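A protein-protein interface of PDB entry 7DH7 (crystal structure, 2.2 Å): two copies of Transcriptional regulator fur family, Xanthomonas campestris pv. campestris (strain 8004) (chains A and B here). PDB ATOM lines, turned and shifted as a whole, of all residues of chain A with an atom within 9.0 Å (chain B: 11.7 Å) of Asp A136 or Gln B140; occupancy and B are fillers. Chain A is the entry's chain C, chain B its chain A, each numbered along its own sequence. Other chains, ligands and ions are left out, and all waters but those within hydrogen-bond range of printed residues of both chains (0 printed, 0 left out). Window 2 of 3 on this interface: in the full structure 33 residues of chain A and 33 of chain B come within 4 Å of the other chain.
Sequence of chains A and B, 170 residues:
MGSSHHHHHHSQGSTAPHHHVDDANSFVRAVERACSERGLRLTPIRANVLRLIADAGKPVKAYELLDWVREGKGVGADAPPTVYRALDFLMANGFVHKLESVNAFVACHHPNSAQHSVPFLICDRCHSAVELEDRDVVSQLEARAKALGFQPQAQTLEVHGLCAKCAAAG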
ATOM      1  N   LEU A 121      -3.783 -31.168  -8.741  1.00  0.00           N
ATOM      2  CA  LEU A 121      -3.606 -29.765  -9.164  1.00  0.00           C
ATOM      3  C   LEU A 121      -4.225 -28.904  -8.056  1.00  0.00           C
ATOM      4  O   LEU A 121      -5.421 -29.031  -7.863  1.00  0.00           O
ATOM      5  CB  LEU A 121      -4.339 -29.639 -10.495  1.00  0.00           C
ATOM      6  CG  LEU A 121      -4.328 -28.272 -11.153  1.00  0.00           C
ATOM      7  CD1 LEU A 121      -2.910 -27.748 -11.272  1.00  0.00           C
ATOM      8  CD2 LEU A 121      -4.973 -28.355 -12.520  1.00  0.00           C
ATOM      9  N   LEU A 132      -5.723 -34.918 -11.855  1.00  0.00           N
ATOM     10  CA  LEU A 132      -5.462 -34.839 -13.289  1.00  0.00           C
ATOM     11  C   LEU A 132      -5.754 -36.209 -13.879  1.00  0.00           C
ATOM     12  O   LEU A 132      -4.912 -37.107 -13.829  1.00  0.00           O
ATOM     13  CB  LEU A 132      -4.024 -34.408 -13.552  1.00  0.00           C
ATOM     14  CG  LEU A 132      -3.860 -32.891 -13.665  1.00  0.00           C
ATOM     15  CD1 LEU A 132      -2.414 -32.440 -13.482  1.00  0.00           C
ATOM     16  CD2 LEU A 132      -4.421 -32.432 -15.008  1.00  0.00           C
ATOM     17  N   GLU A 133      -6.952 -36.381 -14.435  1.00  0.00           N
ATOM     18  CA  GLU A 133      -7.366 -37.680 -14.953  1.00  0.00           C
ATOM     19  C   GLU A 133      -7.071 -37.849 -16.437  1.00  0.00           C
ATOM     20  O   GLU A 133      -7.522 -38.831 -17.034  1.00  0.00           O
ATOM     21  CB  GLU A 133      -8.856 -37.909 -14.676  1.00  0.00           C
ATOM     22  CG  GLU A 133      -9.154 -38.161 -13.208  1.00  0.00           C
ATOM     23  CD  GLU A 133     -10.617 -37.949 -12.860  1.00  0.00           C
ATOM     24  OE1 GLU A 133     -11.397 -37.567 -13.762  1.00  0.00           O
ATOM     25  OE2 GLU A 133     -10.979 -38.132 -11.676  1.00  0.00           O
ATOM     26  N   ASP A 134      -6.328 -36.924 -17.042  1.00  0.00           N
ATOM     27  CA  ASP A 134      -5.944 -37.032 -18.449  1.00  0.00           C
ATOM     28  C   ASP A 134      -4.684 -37.883 -18.501  1.00  0.00           C
ATOM     29  O   ASP A 134      -3.588 -37.419 -18.169  1.00  0.00           O
ATOM     30  CB  ASP A 134      -5.737 -35.652 -19.065  1.00  0.00           C
ATOM     31  CG  ASP A 134      -5.432 -35.706 -20.558  1.00  0.00           C
ATOM     32  OD1 ASP A 134      -5.019 -36.775 -21.065  1.00  0.00           O
ATOM     33  OD2 ASP A 134      -5.619 -34.668 -21.234  1.00  0.00           O
ATOM     34  N   ARG A 135      -4.847 -39.143 -18.918  1.00  0.00           N
ATOM     35  CA  ARG A 135      -3.724 -40.074 -18.951  1.00  0.00           C
ATOM     36  C   ARG A 135      -2.672 -39.615 -19.952  1.00  0.00           C
ATOM     37  O   ARG A 135      -1.467 -39.725 -19.697  1.00  0.00           O
ATOM     38  CB  ARG A 135      -4.212 -41.487 -19.292  1.00  0.00           C
ATOM     39  CG  ARG A 135      -5.234 -42.119 -18.324  1.00  0.00           C
ATOM     40  CD  ARG A 135      -6.676 -41.606 -18.515  1.00  0.00           C
ATOM     41  NE  ARG A 135      -7.031 -41.376 -19.921  1.00  0.00           N
ATOM     42  CZ  ARG A 135      -7.710 -40.318 -20.367  1.00  0.00           C
ATOM     43  NH1 ARG A 135      -8.113 -39.374 -19.528  1.00  0.00           N
ATOM     44  NH2 ARG A 135      -7.984 -40.200 -21.658  1.00  0.00           N
ATOM     45  N   ASP A 136      -3.112 -39.071 -21.083  1.00  0.00           N
ATOM     46  CA  ASP A 136      -2.183 -38.605 -22.107  1.00  0.00           C
ATOM     47  C   ASP A 136      -1.304 -37.476 -21.579  1.00  0.00           C
ATOM     48  O   ASP A 136      -0.077 -37.501 -21.732  1.00  0.00           O
ATOM     49  CB  ASP A 136      -2.975 -38.161 -23.340  1.00  0.00           C
ATOM     50  CG  ASP A 136      -2.137 -37.400 -24.334  1.00  0.00           C
ATOM     51  OD1 ASP A 136      -0.985 -37.817 -24.576  1.00  0.00           O
ATOM     52  OD2 ASP A 136      -2.638 -36.396 -24.886  1.00  0.00           O
ATOM     53  N   VAL A 137      -1.917 -36.474 -20.948  1.00  0.00           N
ATOM     54  CA  VAL A 137      -1.148 -35.343 -20.439  1.00  0.00           C
ATOM     55  C   VAL A 137      -0.284 -35.760 -19.251  1.00  0.00           C
ATOM     56  O   VAL A 137       0.854 -35.297 -19.106  1.00  0.00           O
ATOM     57  CB  VAL A 137      -2.094 -34.181 -20.085  1.00  0.00           C
ATOM     58  CG1 VAL A 137      -1.386 -33.151 -19.225  1.00  0.00           C
ATOM     59  CG2 VAL A 137      -2.632 -33.537 -21.361  1.00  0.00           C
ATOM     60  N   VAL A 138      -0.798 -36.636 -18.384  1.00  0.00           N
ATOM     61  CA  VAL A 138       0.000 -37.087 -17.245  1.00  0.00           C
ATOM     62  C   VAL A 138       1.204 -37.883 -17.732  1.00  0.00           C
ATOM     63  O   VAL A 138       2.327 -37.699 -17.248  1.00  0.00           O
ATOM     64  CB  VAL A 138      -0.862 -37.908 -16.260  1.00  0.00           C
ATOM     65  CG1 VAL A 138       0.016 -38.672 -15.269  1.00  0.00           C
ATOM     66  CG2 VAL A 138      -1.836 -37.004 -15.502  1.00  0.00           C
ATOM     67  N   SER A 139       0.990 -38.763 -18.711  1.00  0.00           N
ATOM     68  CA  SER A 139       2.070 -39.609 -19.211  1.00  0.00           C
ATOM     69  C   SER A 139       3.219 -38.776 -19.756  1.00  0.00           C
ATOM     70  O   SER A 139       4.390 -39.056 -19.470  1.00  0.00           O
ATOM     71  CB  SER A 139       1.536 -40.546 -20.295  1.00  0.00           C
ATOM     72  OG  SER A 139       2.259 -41.762 -20.313  1.00  0.00           O
ATOM     73  N   GLN A 140       2.904 -37.744 -20.541  1.00  0.00           N
ATOM     74  CA  GLN A 140       3.942 -36.865 -21.075  1.00  0.00           C
ATOM     75  C   GLN A 140       4.671 -36.125 -19.961  1.00  0.00           C
ATOM     76  O   GLN A 140       5.908 -36.035 -19.974  1.00  0.00           O
ATOM     77  CB  GLN A 140       3.325 -35.866 -22.055  1.00  0.00           C
ATOM     78  CG  GLN A 140       3.393 -36.282 -23.520  1.00  0.00           C
ATOM     79  CD  GLN A 140       2.296 -35.653 -24.358  1.00  0.00           C
ATOM     80  OE1 GLN A 140       1.175 -36.152 -24.400  1.00  0.00           O
ATOM     81  NE2 GLN A 140       2.612 -34.541 -25.017  1.00  0.00           N
ATOM     82  N   LEU A 141       3.927 -35.580 -18.994  1.00  0.00           N
ATOM     83  CA  LEU A 141       4.556 -34.838 -17.905  1.00  0.00           C
ATOM     84  C   LEU A 141       5.546 -35.718 -17.151  1.00  0.00           C
ATOM     85  O   LEU A 141       6.696 -35.327 -16.934  1.00  0.00           O
ATOM     86  CB  LEU A 141       3.494 -34.285 -16.953  1.00  0.00           C
ATOM     87  CG  LEU A 141       4.048 -33.484 -15.768  1.00  0.00           C
ATOM     88  CD1 LEU A 141       4.707 -32.188 -16.242  1.00  0.00           C
ATOM     89  CD2 LEU A 141       2.964 -33.202 -14.722  1.00  0.00           C
ATOM     90  N   GLU A 142       5.117 -36.926 -16.768  1.00  0.00           N
ATOM     91  CA  GLU A 142       6.009 -37.843 -16.065  1.00  0.00           C
ATOM     92  C   GLU A 142       7.207 -38.212 -16.932  1.00  0.00           C
ATOM     93  O   GLU A 142       8.337 -38.312 -16.437  1.00  0.00           O
ATOM     94  CB  GLU A 142       5.237 -39.089 -15.620  1.00  0.00           C
ATOM     95  CG  GLU A 142       4.296 -38.820 -14.439  1.00  0.00           C
ATOM     96  CD  GLU A 142       3.381 -39.996 -14.097  1.00  0.00           C
ATOM     97  OE1 GLU A 142       3.234 -40.901 -14.943  1.00  0.00           O
ATOM     98  OE2 GLU A 142       2.812 -40.014 -12.974  1.00  0.00           O
ATOM     99  N   ALA A 143       6.986 -38.385 -18.236  1.00  0.00           N
ATOM    100  CA  ALA A 143       8.096 -38.646 -19.147  1.00  0.00           C
ATOM    101  C   ALA A 143       9.085 -37.485 -19.149  1.00  0.00           C
ATOM    102  O   ALA A 143      10.303 -37.694 -19.093  1.00  0.00           O
ATOM    103  CB  ALA A 143       7.565 -38.922 -20.557  1.00  0.00           C
ATOM    104  N   PRO B 119       7.131 -22.983 -16.646  1.00  0.00           N
ATOM    105  CA  PRO B 119       6.938 -23.731 -15.395  1.00  0.00           C
ATOM    106  C   PRO B 119       8.247 -24.268 -14.821  1.00  0.00           C
ATOM    107  O   PRO B 119       9.173 -24.632 -15.549  1.00  0.00           O
ATOM    108  CB  PRO B 119       6.003 -24.872 -15.806  1.00  0.00           C
ATOM    109  CG  PRO B 119       5.265 -24.339 -16.962  1.00  0.00           C
ATOM    110  CD  PRO B 119       6.268 -23.515 -17.719  1.00  0.00           C
ATOM    111  N   LEU B 132      10.805 -26.437 -17.115  1.00  0.00           N
ATOM    112  CA  LEU B 132      10.153 -27.303 -18.100  1.00  0.00           C
ATOM    113  C   LEU B 132      10.108 -26.562 -19.422  1.00  0.00           C
ATOM    114  O   LEU B 132       9.280 -25.672 -19.604  1.00  0.00           O
ATOM    115  CB  LEU B 132       8.739 -27.668 -17.661  1.00  0.00           C
ATOM    116  CG  LEU B 132       8.466 -28.730 -16.599  1.00  0.00           C
ATOM    117  CD1 LEU B 132       6.988 -28.662 -16.249  1.00  0.00           C
ATOM    118  CD2 LEU B 132       8.815 -30.127 -17.069  1.00  0.00           C
ATOM    119  N   GLU B 133      10.992 -26.919 -20.356  1.00  0.00           N
ATOM    120  CA  GLU B 133      11.131 -26.167 -21.599  1.00  0.00           C
ATOM    121  C   GLU B 133      10.516 -26.889 -22.803  1.00  0.00           C
ATOM    122  O   GLU B 133      10.772 -26.503 -23.949  1.00  0.00           O
ATOM    123  CB  GLU B 133      12.606 -25.828 -21.843  1.00  0.00           C
ATOM    124  CG  GLU B 133      13.234 -24.957 -20.732  1.00  0.00           C
ATOM    125  CD  GLU B 133      14.578 -24.330 -21.115  1.00  0.00           C
ATOM    126  OE1 GLU B 133      14.964 -24.402 -22.305  1.00  0.00           O
ATOM    127  OE2 GLU B 133      15.256 -23.765 -20.221  1.00  0.00           O
ATOM    128  N   ASP B 134       9.683 -27.908 -22.566  1.00  0.00           N
ATOM    129  CA  ASP B 134       8.960 -28.622 -23.625  1.00  0.00           C
ATOM    130  C   ASP B 134       7.647 -27.888 -23.874  1.00  0.00           C
ATOM    131  O   ASP B 134       6.659 -28.095 -23.160  1.00  0.00           O
ATOM    132  CB  ASP B 134       8.734 -30.080 -23.229  1.00  0.00           C
ATOM    133  CG  ASP B 134       8.019 -30.890 -24.302  1.00  0.00           C
ATOM    134  OD1 ASP B 134       7.387 -30.307 -25.207  1.00  0.00           O
ATOM    135  OD2 ASP B 134       8.089 -32.133 -24.241  1.00  0.00           O
ATOM    136  N   ARG B 135       7.622 -27.068 -24.932  1.00  0.00           N
ATOM    137  CA  ARG B 135       6.532 -26.113 -25.110  1.00  0.00           C
ATOM    138  C   ARG B 135       5.182 -26.794 -25.300  1.00  0.00           C
ATOM    139  O   ARG B 135       4.156 -26.245 -24.880  1.00  0.00           O
ATOM    140  CB  ARG B 135       6.827 -25.188 -26.284  1.00  0.00           C
ATOM    141  CG  ARG B 135       7.378 -23.841 -25.854  1.00  0.00           C
ATOM    142  CD  ARG B 135       8.866 -23.940 -25.543  1.00  0.00           C
ATOM    143  NE  ARG B 135       9.580 -22.693 -25.803  1.00  0.00           N
ATOM    144  CZ  ARG B 135      10.703 -22.346 -25.185  1.00  0.00           C
ATOM    145  NH1 ARG B 135      11.228 -23.164 -24.282  1.00  0.00           N
ATOM    146  NH2 ARG B 135      11.301 -21.195 -25.471  1.00  0.00           N
ATOM    147  N   ASP B 136       5.146 -27.979 -25.907  1.00  0.00           N
ATOM    148  CA  ASP B 136       3.851 -28.613 -26.130  1.00  0.00           C
ATOM    149  C   ASP B 136       3.356 -29.401 -24.920  1.00  0.00           C
ATOM    150  O   ASP B 136       2.139 -29.482 -24.698  1.00  0.00           O
ATOM    151  CB  ASP B 136       3.897 -29.526 -27.359  1.00  0.00           C
ATOM    152  CG  ASP B 136       2.501 -29.904 -27.852  1.00  0.00           C
ATOM    153  OD1 ASP B 136       1.698 -28.983 -28.136  1.00  0.00           O
ATOM    154  OD2 ASP B 136       2.201 -31.113 -27.957  1.00  0.00           O
ATOM    155  N   VAL B 137       4.260 -29.995 -24.137  1.00  0.00           N
ATOM    156  CA  VAL B 137       3.841 -30.596 -22.875  1.00  0.00           C
ATOM    157  C   VAL B 137       3.255 -29.525 -21.961  1.00  0.00           C
ATOM    158  O   VAL B 137       2.162 -29.687 -21.403  1.00  0.00           O
ATOM    159  CB  VAL B 137       5.016 -31.336 -22.208  1.00  0.00           C
ATOM    160  CG1 VAL B 137       4.712 -31.595 -20.749  1.00  0.00           C
ATOM    161  CG2 VAL B 137       5.274 -32.656 -22.921  1.00  0.00           C
ATOM    162  N   VAL B 138       3.953 -28.392 -21.836  1.00  0.00           N
ATOM    163  CA  VAL B 138       3.447 -27.293 -21.016  1.00  0.00           C
ATOM    164  C   VAL B 138       2.088 -26.825 -21.522  1.00  0.00           C
ATOM    165  O   VAL B 138       1.124 -26.719 -20.755  1.00  0.00           O
ATOM    166  CB  VAL B 138       4.457 -26.138 -20.982  1.00  0.00           C
ATOM    167  CG1 VAL B 138       3.849 -24.943 -20.272  1.00  0.00           C
ATOM    168  CG2 VAL B 138       5.724 -26.590 -20.273  1.00  0.00           C
ATOM    169  N   SER B 139       1.990 -26.557 -22.826  1.00  0.00           N
ATOM    170  CA  SER B 139       0.751 -26.039 -23.401  1.00  0.00           C
ATOM    171  C   SER B 139      -0.422 -26.974 -23.144  1.00  0.00           C
ATOM    172  O   SER B 139      -1.529 -26.524 -22.836  1.00  0.00           O
ATOM    173  CB  SER B 139       0.942 -25.806 -24.902  1.00  0.00           C
ATOM    174  OG  SER B 139      -0.247 -25.319 -25.498  1.00  0.00           O
ATOM    175  N   GLN B 140      -0.199 -28.282 -23.266  1.00  0.00           N
ATOM    176  CA  GLN B 140      -1.236 -29.244 -22.917  1.00  0.00           C
ATOM    177  C   GLN B 140      -1.567 -29.180 -21.430  1.00  0.00           C
ATOM    178  O   GLN B 140      -2.743 -29.167 -21.039  1.00  0.00           O
ATOM    179  CB  GLN B 140      -0.784 -30.649 -23.303  1.00  0.00           C
ATOM    180  CG  GLN B 140      -1.471 -31.238 -24.521  1.00  0.00           C
ATOM    181  CD  GLN B 140      -0.735 -32.447 -25.053  1.00  0.00           C
ATOM    182  OE1 GLN B 140       0.465 -32.384 -25.345  1.00  0.00           O
ATOM    183  NE2 GLN B 140      -1.436 -33.575 -25.135  1.00  0.00           N
ATOM    184  N   LEU B 141      -0.535 -29.154 -20.579  1.00  0.00           N
ATOM    185  CA  LEU B 141      -0.781 -29.058 -19.146  1.00  0.00           C
ATOM    186  C   LEU B 141      -1.587 -27.811 -18.832  1.00  0.00           C
ATOM    187  O   LEU B 141      -2.595 -27.873 -18.115  1.00  0.00           O
ATOM    188  CB  LEU B 141       0.540 -29.059 -18.367  1.00  0.00           C
ATOM    189  CG  LEU B 141       0.353 -28.945 -16.856  1.00  0.00           C
ATOM    190  CD1 LEU B 141      -0.476 -30.130 -16.366  1.00  0.00           C
ATOM    191  CD2 LEU B 141       1.691 -28.876 -16.111  1.00  0.00           C
ATOM    192  N   GLU B 142      -1.176 -26.668 -19.395  1.00  0.00           N
ATOM    193  CA  GLU B 142      -1.884 -25.423 -19.121  1.00  0.00           C
ATOM    194  C   GLU B 142      -3.338 -25.494 -19.577  1.00  0.00           C
ATOM    195  O   GLU B 142      -4.225 -24.968 -18.894  1.00  0.00           O
ATOM    196  CB  GLU B 142      -1.172 -24.250 -19.780  1.00  0.00           C
ATOM    197  CG  GLU B 142       0.232 -24.034 -19.270  1.00  0.00           C
ATOM    198  CD  GLU B 142       0.945 -22.915 -19.989  1.00  0.00           C
ATOM    199  OE1 GLU B 142       0.635 -22.673 -21.177  1.00  0.00           O
ATOM    200  OE2 GLU B 142       1.812 -22.274 -19.370  1.00  0.00           O
ATOM    201  N   ALA B 143      -3.599 -26.140 -20.728  1.00  0.00           N
ATOM    202  CA  ALA B 143      -4.973 -26.277 -21.216  1.00  0.00           C
ATOM    203  C   ALA B 143      -5.815 -27.099 -20.252  1.00  0.00           C
ATOM    204  O   ALA B 143      -6.935 -26.711 -19.904  1.00  0.00           O
ATOM    205  CB  ALA B 143      -4.998 -26.912 -22.613  1.00  0.00           C
ATOM    206  N   ARG B 144      -5.294 -28.250 -19.823  1.00  0.00           N
ATOM    207  CA  ARG B 144      -5.983 -29.049 -18.819  1.00  0.00           C
ATOM    208  C   ARG B 144      -6.334 -28.220 -17.583  1.00  0.00           C
ATOM    209  O   ARG B 144      -7.469 -28.274 -17.097  1.00  0.00           O
ATOM    210  CB  ARG B 144      -5.122 -30.256 -18.437  1.00  0.00           C
ATOM    211  CG  ARG B 144      -5.255 -31.432 -19.384  1.00  0.00           C
ATOM    212  CD  ARG B 144      -6.648 -32.041 -19.299  1.00  0.00           C
ATOM    213  NE  ARG B 144      -7.566 -31.386 -20.225  1.00  0.00           N
ATOM    214  CZ  ARG B 144      -8.813 -31.025 -19.923  1.00  0.00           C
ATOM    215  NH1 ARG B 144      -9.305 -31.252 -18.711  1.00  0.00           N
ATOM    216  NH2 ARG B 144      -9.567 -30.429 -20.841  1.00  0.00           N
ATOM    217  N   ALA B 145      -5.391 -27.405 -17.099  1.00  0.00           N
ATOM    218  CA  ALA B 145      -5.599 -26.674 -15.851  1.00  0.00           C
ATOM    219  C   ALA B 145      -6.622 -25.549 -16.012  1.00  0.00           C
ATOM    220  O   ALA B 145      -7.407 -25.282 -15.097  1.00  0.00           O
ATOM    221  CB  ALA B 145      -4.262 -26.121 -15.339  1.00  0.00           C
ATOM    222  N   LYS B 146      -6.607 -24.852 -17.151  1.00  0.00           N
ATOM    223  CA  LYS B 146      -7.630 -23.840 -17.402  1.00  0.00           C
ATOM    224  C   LYS B 146      -9.022 -24.467 -17.393  1.00  0.00           C
ATOM    225  O   LYS B 146      -9.939 -23.975 -16.721  1.00  0.00           O
ATOM    226  CB  LYS B 146      -7.351 -23.140 -18.735  1.00  0.00           C
ATOM    227  CG  LYS B 146      -8.422 -22.144 -19.169  1.00  0.00           C
ATOM    228  CD  LYS B 146      -9.080 -22.547 -20.495  1.00  0.00           C
ATOM    229  CE  LYS B 146      -9.646 -21.335 -21.251  1.00  0.00           C
ATOM    230  NZ  LYS B 146     -10.543 -21.701 -22.404  1.00  0.00           N
ATOM    231  N   ALA B 147      -9.179 -25.582 -18.114  1.00  0.00           N
ATOM    232  CA  ALA B 147     -10.457 -26.279 -18.159  1.00  0.00           C
ATOM    233  C   ALA B 147     -10.916 -26.682 -16.766  1.00  0.00           C
ATOM    234  O   ALA B 147     -12.118 -26.666 -16.471  1.00  0.00           O
ATOM    235  CB  ALA B 147     -10.351 -27.508 -19.066  1.00  0.00           C
ATOM    236  N   LEU B 148      -9.973 -27.032 -15.892  1.00  0.00           N
ATOM    237  CA  LEU B 148     -10.274 -27.492 -14.546  1.00  0.00           C
ATOM    238  C   LEU B 148     -10.406 -26.354 -13.546  1.00  0.00           C
ATOM    239  O   LEU B 148     -10.530 -26.616 -12.347  1.00  0.00           O
ATOM    240  CB  LEU B 148      -9.201 -28.471 -14.081  1.00  0.00           C
ATOM    241  CG  LEU B 148      -9.161 -29.822 -14.796  1.00  0.00           C
ATOM    242  CD1 LEU B 148      -7.929 -30.597 -14.377  1.00  0.00           C
ATOM    243  CD2 LEU B 148     -10.419 -30.638 -14.532  1.00  0.00           C
ATOM    244  N   GLY B 149     -10.375 -25.103 -13.994  1.00  0.00           N
ATOM    245  CA  GLY B 149     -10.664 -23.992 -13.117  1.00  0.00           C
ATOM    246  C   GLY B 149      -9.489 -23.161 -12.656  1.00  0.00           C
ATOM    247  O   GLY B 149      -9.671 -22.312 -11.771  1.00  0.00           O
ATOM    248  N   PHE B 150      -8.296 -23.378 -13.213  1.00  0.00           N
ATOM    249  CA  PHE B 150      -7.109 -22.609 -12.867  1.00  0.00           C
ATOM    250  C   PHE B 150      -6.829 -21.549 -13.926  1.00  0.00           C
ATOM    251  O   PHE B 150      -7.380 -21.579 -15.031  1.00  0.00           O
ATOM    252  CB  PHE B 150      -5.896 -23.540 -12.688  1.00  0.00           C
ATOM    253  CG  PHE B 150      -5.958 -24.365 -11.420  1.00  0.00           C
ATOM    254  CD1 PHE B 150      -6.807 -25.457 -11.314  1.00  0.00           C
ATOM    255  CD2 PHE B 150      -5.188 -24.021 -10.322  1.00  0.00           C
ATOM    256  CE1 PHE B 150      -6.869 -26.206 -10.128  1.00  0.00           C
ATOM    257  CE2 PHE B 150      -5.240 -24.754  -9.163  1.00  0.00           C
ATOM    258  CZ  PHE B 150      -6.084 -25.846  -9.052  1.00  0.00           C
ATOM    259  N   GLN B 151      -5.936 -20.608 -13.580  1.00  0.00           N
ATOM    260  CA  GLN B 151      -5.532 -19.517 -14.470  1.00  0.00           C
ATOM    261  C   GLN B 151      -4.038 -19.607 -14.731  1.00  0.00           C
ATOM    262  O   GLN B 151      -3.254 -18.834 -14.167  1.00  0.00           O
ATOM    263  CB  GLN B 151      -5.871 -18.151 -13.888  1.00  0.00           C
ATOM    264  CG  GLN B 151      -7.315 -18.012 -13.562  1.00  0.00           C
ATOM    265  CD  GLN B 151      -8.082 -17.219 -14.603  1.00  0.00           C
ATOM    266  OE1 GLN B 151      -7.790 -17.291 -15.800  1.00  0.00           O
ATOM    267  NE2 GLN B 151      -9.103 -16.491 -14.153  1.00  0.00           N
ATOM    268  N   PRO B 152      -3.614 -20.505 -15.620  1.00  0.00           N
ATOM    269  CA  PRO B 152      -2.172 -20.685 -15.861  1.00  0.00           C
ATOM    270  C   PRO B 152      -1.451 -19.423 -16.337  1.00  0.00           C
ATOM    271  O   PRO B 152      -0.213 -19.428 -16.379  1.00  0.00           O
ATOM    272  CB  PRO B 152      -2.125 -21.781 -16.939  1.00  0.00           C
ATOM    273  CG  PRO B 152      -3.534 -22.355 -17.007  1.00  0.00           C
ATOM    274  CD  PRO B 152      -4.447 -21.263 -16.567  1.00  0.00           C
ATOM    275  N   GLN B 153      -2.165 -18.355 -16.704  1.00  0.00           N
ATOM    276  CA  GLN B 153      -1.513 -17.124 -17.133  1.00  0.00           C
ATOM    277  C   GLN B 153      -1.545 -16.016 -16.084  1.00  0.00           C
ATOM    278  O   GLN B 153      -0.853 -15.008 -16.255  1.00  0.00           O
ATOM    279  CB  GLN B 153      -2.128 -16.610 -18.445  1.00  0.00           C
ATOM    280  CG  GLN B 153      -2.090 -17.623 -19.598  1.00  0.00           C
ATOM    281  CD  GLN B 153      -0.679 -17.992 -20.041  1.00  0.00           C
ATOM    282  OE1 GLN B 153       0.161 -17.126 -20.294  1.00  0.00           O
ATOM    283  NE2 GLN B 153      -0.417 -19.290 -20.141  1.00  0.00           N
ATOM    284  N   LEU B 157       2.495 -22.113 -13.672  1.00  0.00           N
ATOM    285  CA  LEU B 157       2.367 -23.323 -12.872  1.00  0.00           C
ATOM    286  C   LEU B 157       3.724 -23.805 -12.343  1.00  0.00           C
ATOM    287  O   LEU B 157       4.786 -23.526 -12.910  1.00  0.00           O
ATOM    288  CB  LEU B 157       1.726 -24.434 -13.706  1.00  0.00           C
ATOM    289  CG  LEU B 157       0.309 -24.193 -14.242  1.00  0.00           C
ATOM    290  CD1 LEU B 157      -0.118 -25.360 -15.125  1.00  0.00           C
ATOM    291  CD2 LEU B 157      -0.702 -23.958 -13.111  1.00  0.00           C
ATOM    292  N   VAL B 159       5.444 -27.619 -10.932  1.00  0.00           N
ATOM    293  CA  VAL B 159       5.344 -29.055 -10.707  1.00  0.00           C
ATOM    294  C   VAL B 159       6.255 -29.406  -9.533  1.00  0.00           C
ATOM    295  O   VAL B 159       7.413 -28.973  -9.487  1.00  0.00           O
ATOM    296  CB  VAL B 159       5.717 -29.840 -11.973  1.00  0.00           C
ATOM    297  CG1 VAL B 159       5.466 -31.315 -11.791  1.00  0.00           C
ATOM    298  CG2 VAL B 159       4.949 -29.299 -13.170  1.00  0.00           C
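Asp A136 touches Gln B140, but with the chains exchanged Gln A140 does not touch Asp B136 (4.5 Å). Val A137 touches Gln B140, and with the chains exchanged Gln A140 touches Val B137. Gln A140 touches its own counterpart, Gln B140.
The side-chain carboxylate of Asp B134 is in hydrogen-bond range of the backbone NH of Val B137, at 3.3 Å. OE1 of Gln B140 lies close to OD2 of Asp B136 (3.4 Å). The backbone carbonyl oxygen (O) of Ala B145 sits at hydrogen-bond distance from the backbone NH (N) of Phe B150, 2.8 Å away. The side-chain carboxylate (OD1) of Asp A134 sits at hydrogen-bond distance from the backbone NH (N) of Asp A136 (3.0 Å). The side-chain carboxylate (OD1) of Asp A134 lies within hydrogen-bond range of the backbone NH (N) of Val A137, at 3.1 Å. OD1 of Asp A136 lies close to OE1 of Gln A140 (2.7 Å).
The side-chain amide nitrogen (NE2) of Gln B140 is in hydrogen-bond range of the side-chain carboxylate (OD2) of Asp A136 (3.1 Å). OE1 of Gln B140 lies within hydrogen-bond range of NE2 of Gln A140, at 3.1 Å. The guanidinium group (NE) of Arg B144 lies within salt-bridge range of the side-chain carboxylate (OD2) of Asp A134, 3.9 Å away.
Hydrophobic or aromatic side chains of chain B within 4 Å of the printed part of chain A: Val B137, Ala B145 and Phe B150. Of the 13 printed residues of chain A, 5 touch a printed residue of chain B. Printed residues of chain A that touch a printed residue of chain B: Leu A121, Asp A134, Asp A136, Val A137 and Gln A140. Hydrophobic or aromatic side chains of chain A that line the printed part of chain B: Leu A121 and Val A137. Among the printed residues, 8 pairs touch across the chains.
Of the printed residues of chain B, Asp A136 touches Gln B140 (3.1 Å). Of chain A, only Asp A136 (3.1 Å), Val A137 (3.9 Å) and Gln A140 (3.1 Å) come within 4 Å of Gln B140. Asp A134 touches just one residue of chain B: Arg B144 (3.4 Å). Arg A135 touches none of the printed residues of chain B. Val A137 touches just these residues of chain B: Gln B140 (3.9 Å) and Arg B144 (3.9 Å). No residue of chain B comes within 4 Å of Val A138. No residue of chain B comes within 4 Å of Ser A139. Of chain B, only Val B137 (3.9 Å) and Gln B140 (3.1 Å) come within 4 Å of Gln A140. No residue of chain A comes within 4 Å of Ser B139. Of the printed residues of chain A, Val B137 touches Gln A140. Of the printed residues of chain B, Leu A121 touches Ala B145 and Phe B150. Of the printed residues of chain A, Ala B145 touches Leu A121 (3.7 Å). Of the printed residues of chain A, Phe B150 touches Leu A121. The nearest residue of chain B that does not touch Asp A136 is Val B137 (7.3 Å). The nearest printed residue of chain B that does not touch Leu A121 is Leu B148 (4.1 Å).
Among the printed residues, pairs that only touch across the chains: Leu A121 with Ala B145, Leu A121 with Phe B150, Val A137 with Gln B140, Val A137 with Arg B144 and Gln A140 with Val B137.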
